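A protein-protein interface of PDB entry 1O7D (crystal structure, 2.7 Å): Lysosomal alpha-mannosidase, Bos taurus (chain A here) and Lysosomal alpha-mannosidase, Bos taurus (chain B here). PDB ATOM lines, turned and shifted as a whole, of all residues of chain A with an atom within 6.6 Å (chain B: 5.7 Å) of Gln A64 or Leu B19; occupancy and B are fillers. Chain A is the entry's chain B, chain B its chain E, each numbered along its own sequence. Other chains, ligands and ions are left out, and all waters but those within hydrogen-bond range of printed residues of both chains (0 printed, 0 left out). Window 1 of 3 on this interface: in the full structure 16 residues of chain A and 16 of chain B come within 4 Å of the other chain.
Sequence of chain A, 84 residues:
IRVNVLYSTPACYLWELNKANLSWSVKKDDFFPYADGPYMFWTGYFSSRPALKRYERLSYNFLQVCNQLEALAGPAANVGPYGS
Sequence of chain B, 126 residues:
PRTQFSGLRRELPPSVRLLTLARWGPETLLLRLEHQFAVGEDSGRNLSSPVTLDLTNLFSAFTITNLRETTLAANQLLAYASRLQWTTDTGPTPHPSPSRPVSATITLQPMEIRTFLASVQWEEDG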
ATOM      1  N   SER A  59      -4.129   1.865  22.195  1.00  0.00           N
ATOM      2  CA  SER A  59      -2.820   1.398  22.626  1.00  0.00           C
ATOM      3  C   SER A  59      -2.072   0.834  21.405  1.00  0.00           C
ATOM      4  O   SER A  59      -0.824   0.846  21.346  1.00  0.00           O
ATOM      5  CB  SER A  59      -2.964   0.333  23.716  1.00  0.00           C
ATOM      6  OG  SER A  59      -3.514   0.875  24.898  1.00  0.00           O
ATOM      7  N   TYR A  60      -2.837   0.347  20.428  1.00  0.00           N
ATOM      8  CA  TYR A  60      -2.243  -0.181  19.210  1.00  0.00           C
ATOM      9  C   TYR A  60      -1.505   0.954  18.478  1.00  0.00           C
ATOM     10  O   TYR A  60      -0.308   0.855  18.187  1.00  0.00           O
ATOM     11  CB  TYR A  60      -3.318  -0.765  18.286  1.00  0.00           C
ATOM     12  CG  TYR A  60      -2.758  -1.232  16.950  1.00  0.00           C
ATOM     13  CD1 TYR A  60      -2.107  -2.466  16.828  1.00  0.00           C
ATOM     14  CD2 TYR A  60      -2.851  -0.419  15.815  1.00  0.00           C
ATOM     15  CE1 TYR A  60      -1.567  -2.870  15.612  1.00  0.00           C
ATOM     16  CE2 TYR A  60      -2.312  -0.816  14.599  1.00  0.00           C
ATOM     17  CZ  TYR A  60      -1.673  -2.041  14.500  1.00  0.00           C
ATOM     18  OH  TYR A  60      -1.155  -2.431  13.286  1.00  0.00           O
ATOM     19  N   ASN A  61      -2.237   2.026  18.187  1.00  0.00           N
ATOM     20  CA  ASN A  61      -1.694   3.185  17.499  1.00  0.00           C
ATOM     21  C   ASN A  61      -0.446   3.622  18.221  1.00  0.00           C
ATOM     22  O   ASN A  61       0.540   4.009  17.602  1.00  0.00           O
ATOM     23  CB  ASN A  61      -2.710   4.328  17.523  1.00  0.00           C
ATOM     24  CG  ASN A  61      -2.362   5.442  16.562  1.00  0.00           C
ATOM     25  OD1 ASN A  61      -3.109   6.409  16.409  1.00  0.00           O
ATOM     26  ND2 ASN A  61      -1.230   5.307  15.899  1.00  0.00           N
ATOM     27  N   PHE A  62      -0.508   3.536  19.546  1.00  0.00           N
ATOM     28  CA  PHE A  62       0.580   3.949  20.415  1.00  0.00           C
ATOM     29  C   PHE A  62       1.795   3.028  20.370  1.00  0.00           C
ATOM     30  O   PHE A  62       2.922   3.500  20.210  1.00  0.00           O
ATOM     31  CB  PHE A  62       0.067   4.082  21.857  1.00  0.00           C
ATOM     32  CG  PHE A  62       1.043   4.746  22.792  1.00  0.00           C
ATOM     33  CD1 PHE A  62       1.373   6.084  22.631  1.00  0.00           C
ATOM     34  CD2 PHE A  62       1.664   4.022  23.805  1.00  0.00           C
ATOM     35  CE1 PHE A  62       2.314   6.691  23.464  1.00  0.00           C
ATOM     36  CE2 PHE A  62       2.609   4.618  24.650  1.00  0.00           C
ATOM     37  CZ  PHE A  62       2.937   5.951  24.478  1.00  0.00           C
ATOM     38  N   LEU A  63       1.573   1.728  20.521  1.00  0.00           N
ATOM     39  CA  LEU A  63       2.669   0.768  20.484  1.00  0.00           C
ATOM     40  C   LEU A  63       3.421   0.914  19.152  1.00  0.00           C
ATOM     41  O   LEU A  63       4.650   0.839  19.096  1.00  0.00           O
ATOM     42  CB  LEU A  63       2.113  -0.652  20.601  1.00  0.00           C
ATOM     43  CG  LEU A  63       2.959  -1.815  21.141  1.00  0.00           C
ATOM     44  CD1 LEU A  63       2.445  -3.084  20.490  1.00  0.00           C
ATOM     45  CD2 LEU A  63       4.424  -1.641  20.843  1.00  0.00           C
ATOM     46  N   GLN A  64       2.662   1.117  18.083  1.00  0.00           N
ATOM     47  CA  GLN A  64       3.217   1.284  16.750  1.00  0.00           C
ATOM     48  C   GLN A  64       4.214   2.429  16.734  1.00  0.00           C
ATOM     49  O   GLN A  64       5.369   2.257  16.355  1.00  0.00           O
ATOM     50  CB  GLN A  64       2.105   1.591  15.762  1.00  0.00           C
ATOM     51  CG  GLN A  64       2.210   0.776  14.520  1.00  0.00           C
ATOM     52  CD  GLN A  64       1.750  -0.640  14.739  1.00  0.00           C
ATOM     53  OE1 GLN A  64       2.097  -1.285  15.742  1.00  0.00           O
ATOM     54  NE2 GLN A  64       0.966  -1.147  13.794  1.00  0.00           N
ATOM     55  N   VAL A  65       3.739   3.605  17.125  1.00  0.00           N
ATOM     56  CA  VAL A  65       4.569   4.786  17.190  1.00  0.00           C
ATOM     57  C   VAL A  65       5.777   4.454  18.039  1.00  0.00           C
ATOM     58  O   VAL A  65       6.889   4.811  17.703  1.00  0.00           O
ATOM     59  CB  VAL A  65       3.790   5.945  17.827  1.00  0.00           C
ATOM     60  CG1 VAL A  65       4.692   7.127  18.045  1.00  0.00           C
ATOM     61  CG2 VAL A  65       2.614   6.328  16.925  1.00  0.00           C
ATOM     62  N   CYS A  66       5.552   3.753  19.142  1.00  0.00           N
ATOM     63  CA  CYS A  66       6.638   3.352  20.035  1.00  0.00           C
ATOM     64  C   CYS A  66       7.632   2.495  19.244  1.00  0.00           C
ATOM     65  O   CYS A  66       8.836   2.744  19.282  1.00  0.00           O
ATOM     66  CB  CYS A  66       6.074   2.564  21.238  1.00  0.00           C
ATOM     67  SG  CYS A  66       7.227   2.082  22.599  1.00  0.00           S
ATOM     68  N   ASN A  67       7.125   1.497  18.520  1.00  0.00           N
ATOM     69  CA  ASN A  67       7.976   0.625  17.719  1.00  0.00           C
ATOM     70  C   ASN A  67       8.783   1.393  16.690  1.00  0.00           C
ATOM     71  O   ASN A  67      10.006   1.259  16.632  1.00  0.00           O
ATOM     72  CB  ASN A  67       7.144  -0.427  16.987  1.00  0.00           C
ATOM     73  CG  ASN A  67       6.782  -1.589  17.870  1.00  0.00           C
ATOM     74  OD1 ASN A  67       7.618  -2.075  18.636  1.00  0.00           O
ATOM     75  ND2 ASN A  67       5.542  -2.051  17.768  1.00  0.00           N
ATOM     76  N   GLN A  68       8.099   2.193  15.874  1.00  0.00           N
ATOM     77  CA  GLN A  68       8.766   2.964  14.836  1.00  0.00           C
ATOM     78  C   GLN A  68       9.880   3.827  15.386  1.00  0.00           C
ATOM     79  O   GLN A  68      10.904   3.965  14.745  1.00  0.00           O
ATOM     80  CB  GLN A  68       7.791   3.867  14.091  1.00  0.00           C
ATOM     81  CG  GLN A  68       6.696   3.184  13.318  1.00  0.00           C
ATOM     82  CD  GLN A  68       6.076   4.104  12.255  1.00  0.00           C
ATOM     83  OE1 GLN A  68       6.149   5.335  12.347  1.00  0.00           O
ATOM     84  NE2 GLN A  68       5.457   3.505  11.252  1.00  0.00           N
ATOM     85  N   LEU A  69       9.699   4.419  16.563  1.00  0.00           N
ATOM     86  CA  LEU A  69      10.754   5.273  17.110  1.00  0.00           C
ATOM     87  C   LEU A  69      11.976   4.508  17.622  1.00  0.00           C
ATOM     88  O   LEU A  69      13.116   4.979  17.511  1.00  0.00           O
ATOM     89  CB  LEU A  69      10.203   6.169  18.225  1.00  0.00           C
ATOM     90  CG  LEU A  69       9.522   7.450  17.745  1.00  0.00           C
ATOM     91  CD1 LEU A  69       9.092   8.262  18.944  1.00  0.00           C
ATOM     92  CD2 LEU A  69      10.475   8.241  16.872  1.00  0.00           C
ATOM     93  N   ARG B  17       0.995   0.591   2.529  1.00  0.00           N
ATOM     94  CA  ARG B  17       0.958   0.950   3.933  1.00  0.00           C
ATOM     95  C   ARG B  17       2.134   0.353   4.704  1.00  0.00           C
ATOM     96  O   ARG B  17       2.467  -0.815   4.535  1.00  0.00           O
ATOM     97  CB  ARG B  17      -0.332   0.463   4.569  1.00  0.00           C
ATOM     98  CG  ARG B  17      -0.370   0.752   6.050  1.00  0.00           C
ATOM     99  CD  ARG B  17      -1.553   0.109   6.695  1.00  0.00           C
ATOM    100  NE  ARG B  17      -2.795   0.566   6.094  1.00  0.00           N
ATOM    101  CZ  ARG B  17      -3.975   0.441   6.680  1.00  0.00           C
ATOM    102  NH1 ARG B  17      -4.064  -0.122   7.875  1.00  0.00           N
ATOM    103  NH2 ARG B  17      -5.059   0.882   6.072  1.00  0.00           N
ATOM    104  N   LEU B  18       2.777   1.162   5.540  1.00  0.00           N
ATOM    105  CA  LEU B  18       3.876   0.666   6.349  1.00  0.00           C
ATOM    106  C   LEU B  18       3.175  -0.012   7.502  1.00  0.00           C
ATOM    107  O   LEU B  18       2.696   0.644   8.411  1.00  0.00           O
ATOM    108  CB  LEU B  18       4.754   1.807   6.877  1.00  0.00           C
ATOM    109  CG  LEU B  18       5.917   1.434   7.808  1.00  0.00           C
ATOM    110  CD1 LEU B  18       6.913   0.549   7.066  1.00  0.00           C
ATOM    111  CD2 LEU B  18       6.622   2.694   8.309  1.00  0.00           C
ATOM    112  N   LEU B  19       3.094  -1.332   7.443  1.00  0.00           N
ATOM    113  CA  LEU B  19       2.430  -2.096   8.482  1.00  0.00           C
ATOM    114  C   LEU B  19       3.237  -2.147   9.766  1.00  0.00           C
ATOM    115  O   LEU B  19       2.733  -1.818  10.839  1.00  0.00           O
ATOM    116  CB  LEU B  19       2.158  -3.514   7.998  1.00  0.00           C
ATOM    117  CG  LEU B  19       1.383  -4.376   8.988  1.00  0.00           C
ATOM    118  CD1 LEU B  19       0.207  -3.594   9.562  1.00  0.00           C
ATOM    119  CD2 LEU B  19       0.909  -5.629   8.289  1.00  0.00           C
ATOM    120  N   THR B  20       4.493  -2.550   9.675  1.00  0.00           N
ATOM    121  CA  THR B  20       5.294  -2.630  10.872  1.00  0.00           C
ATOM    122  C   THR B  20       6.704  -2.132  10.632  1.00  0.00           C
ATOM    123  O   THR B  20       7.293  -2.378   9.585  1.00  0.00           O
ATOM    124  CB  THR B  20       5.375  -4.087  11.387  1.00  0.00           C
ATOM    125  OG1 THR B  20       4.059  -4.618  11.565  1.00  0.00           O
ATOM    126  CG2 THR B  20       6.088  -4.131  12.712  1.00  0.00           C
ATOM    127  N   LEU B  21       7.222  -1.389  11.596  1.00  0.00           N
ATOM    128  CA  LEU B  21       8.591  -0.911  11.558  1.00  0.00           C
ATOM    129  C   LEU B  21       8.934  -1.195  12.999  1.00  0.00           C
ATOM    130  O   LEU B  21       8.309  -0.641  13.897  1.00  0.00           O
ATOM    131  CB  LEU B  21       8.676   0.587  11.265  1.00  0.00           C
ATOM    132  CG  LEU B  21      10.110   1.136  11.221  1.00  0.00           C
ATOM    133  CD1 LEU B  21      10.948   0.303  10.248  1.00  0.00           C
ATOM    134  CD2 LEU B  21      10.087   2.613  10.829  1.00  0.00           C
ATOM    135  N   ARG B  32       7.108  -4.764   7.714  1.00  0.00           N
ATOM    136  CA  ARG B  32       6.003  -5.348   6.987  1.00  0.00           C
ATOM    137  C   ARG B  32       5.402  -4.257   6.127  1.00  0.00           C
ATOM    138  O   ARG B  32       5.234  -3.132   6.571  1.00  0.00           O
ATOM    139  CB  ARG B  32       4.953  -5.909   7.942  1.00  0.00           C
ATOM    140  CG  ARG B  32       5.370  -7.194   8.655  1.00  0.00           C
ATOM    141  CD  ARG B  32       4.141  -7.988   9.101  1.00  0.00           C
ATOM    142  NE  ARG B  32       4.453  -9.116   9.982  1.00  0.00           N
ATOM    143  CZ  ARG B  32       4.547  -9.047  11.312  1.00  0.00           C
ATOM    144  NH1 ARG B  32       4.354  -7.900  11.946  1.00  0.00           N
ATOM    145  NH2 ARG B  32       4.817 -10.137  12.017  1.00  0.00           N
ATOM    146  N   LEU B  33       5.087  -4.587   4.885  1.00  0.00           N
ATOM    147  CA  LEU B  33       4.514  -3.610   3.972  1.00  0.00           C
ATOM    148  C   LEU B  33       3.311  -4.226   3.283  1.00  0.00           C
ATOM    149  O   LEU B  33       3.450  -5.187   2.539  1.00  0.00           O
ATOM    150  CB  LEU B  33       5.548  -3.204   2.920  1.00  0.00           C
ATOM    151  CG  LEU B  33       6.859  -2.600   3.424  1.00  0.00           C
ATOM    152  CD1 LEU B  33       7.911  -2.635   2.313  1.00  0.00           C
ATOM    153  CD2 LEU B  33       6.608  -1.174   3.930  1.00  0.00           C
ATOM    154  N   GLU B  34       2.130  -3.670   3.516  1.00  0.00           N
ATOM    155  CA  GLU B  34       0.938  -4.214   2.900  1.00  0.00           C
ATOM    156  C   GLU B  34       0.354  -3.306   1.848  1.00  0.00           C
ATOM    157  O   GLU B  34       0.607  -2.113   1.812  1.00  0.00           O
ATOM    158  CB  GLU B  34      -0.121  -4.513   3.952  1.00  0.00           C
ATOM    159  CG  GLU B  34      -1.036  -3.361   4.246  1.00  0.00           C
ATOM    160  CD  GLU B  34      -2.025  -3.692   5.344  1.00  0.00           C
ATOM    161  OE1 GLU B  34      -1.562  -4.019   6.458  1.00  0.00           O
ATOM    162  OE2 GLU B  34      -3.254  -3.634   5.102  1.00  0.00           O
ATOM    163  N   LEU B  72       4.139 -14.361   7.469  1.00  0.00           N
ATOM    164  CA  LEU B  72       3.519 -13.293   8.244  1.00  0.00           C
ATOM    165  C   LEU B  72       3.913 -13.147   9.723  1.00  0.00           C
ATOM    166  O   LEU B  72       4.232 -12.048  10.154  1.00  0.00           O
ATOM    167  CB  LEU B  72       1.998 -13.370   8.111  1.00  0.00           C
ATOM    168  CG  LEU B  72       1.185 -12.180   8.622  1.00  0.00           C
ATOM    169  CD1 LEU B  72       1.681 -10.871   8.026  1.00  0.00           C
ATOM    170  CD2 LEU B  72      -0.278 -12.418   8.269  1.00  0.00           C
ATOM    171  N   ILE B 113       0.705  -8.839   1.963  1.00  0.00           N
ATOM    172  CA  ILE B 113       1.535  -8.335   3.055  1.00  0.00           C
ATOM    173  C   ILE B 113       2.844  -9.105   3.038  1.00  0.00           C
ATOM    174  O   ILE B 113       2.848 -10.330   3.157  1.00  0.00           O
ATOM    175  CB  ILE B 113       0.910  -8.595   4.435  1.00  0.00           C
ATOM    176  CG1 ILE B 113      -0.411  -7.838   4.577  1.00  0.00           C
ATOM    177  CG2 ILE B 113       1.909  -8.213   5.522  1.00  0.00           C
ATOM    178  CD1 ILE B 113      -1.187  -8.178   5.844  1.00  0.00           C
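Gln A64 touches one residue of chain B. Leu B19 touches just one residue of chain A: Gln A64 (3.5 Å). Of the printed residues of chain B, Asn A67 touches Leu B21 (3.3 Å). Of the printed residues of chain A, Leu B18 touches Gln A68. Printed residues of chain B within 4 Å of Gln A68: Leu B18 (3.3 Å) and Leu B21 (3.5 Å). Of the printed residues of chain A, Leu B21 touches Asn A67 (3.3 Å) and Gln A68 (3.5 Å). Leu B72 touches none of the printed residues of chain A. Ile B113 touches none of the printed residues of chain A. The nearest residue of chain B that does not touch Gln A64 is Leu B21 (4.8 Å). The nearest residue of chain A that does not touch Leu B19 is Tyr A60 (4.1 Å).
O of Leu B21 sits at hydrogen-bond distance from N of Gln A68, at 3.5 Å.
Of the 11 printed residues of chain A, 3 touch a printed residue of chain B. Printed residues of chain A that touch a printed residue of chain B: Gln A64, Asn A67 and Gln A68. Of the 10 printed residues of chain B, 3 touch a printed residue of chain A. Along chain B the printed residues that touch a printed residue of chain A span positions 18 to 21. Among the printed residues, 4 pairs touch across the chains.
Among the printed residues, pairs that only touch across the chains: Gln A68 with Leu B18, Asn A67 with Leu B21 and Gln A64 with Leu B19.
NE2 of Gln A64 is in hydrogen-bond range of OH of Tyr A60, at 2.5 Å. O of Leu A63 sits close to ND2 of Asn A67 (3.3 Å). The backbone carbonyl oxygen of Arg B32 is in hydrogen-bond range of the backbone NH of Leu B19.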
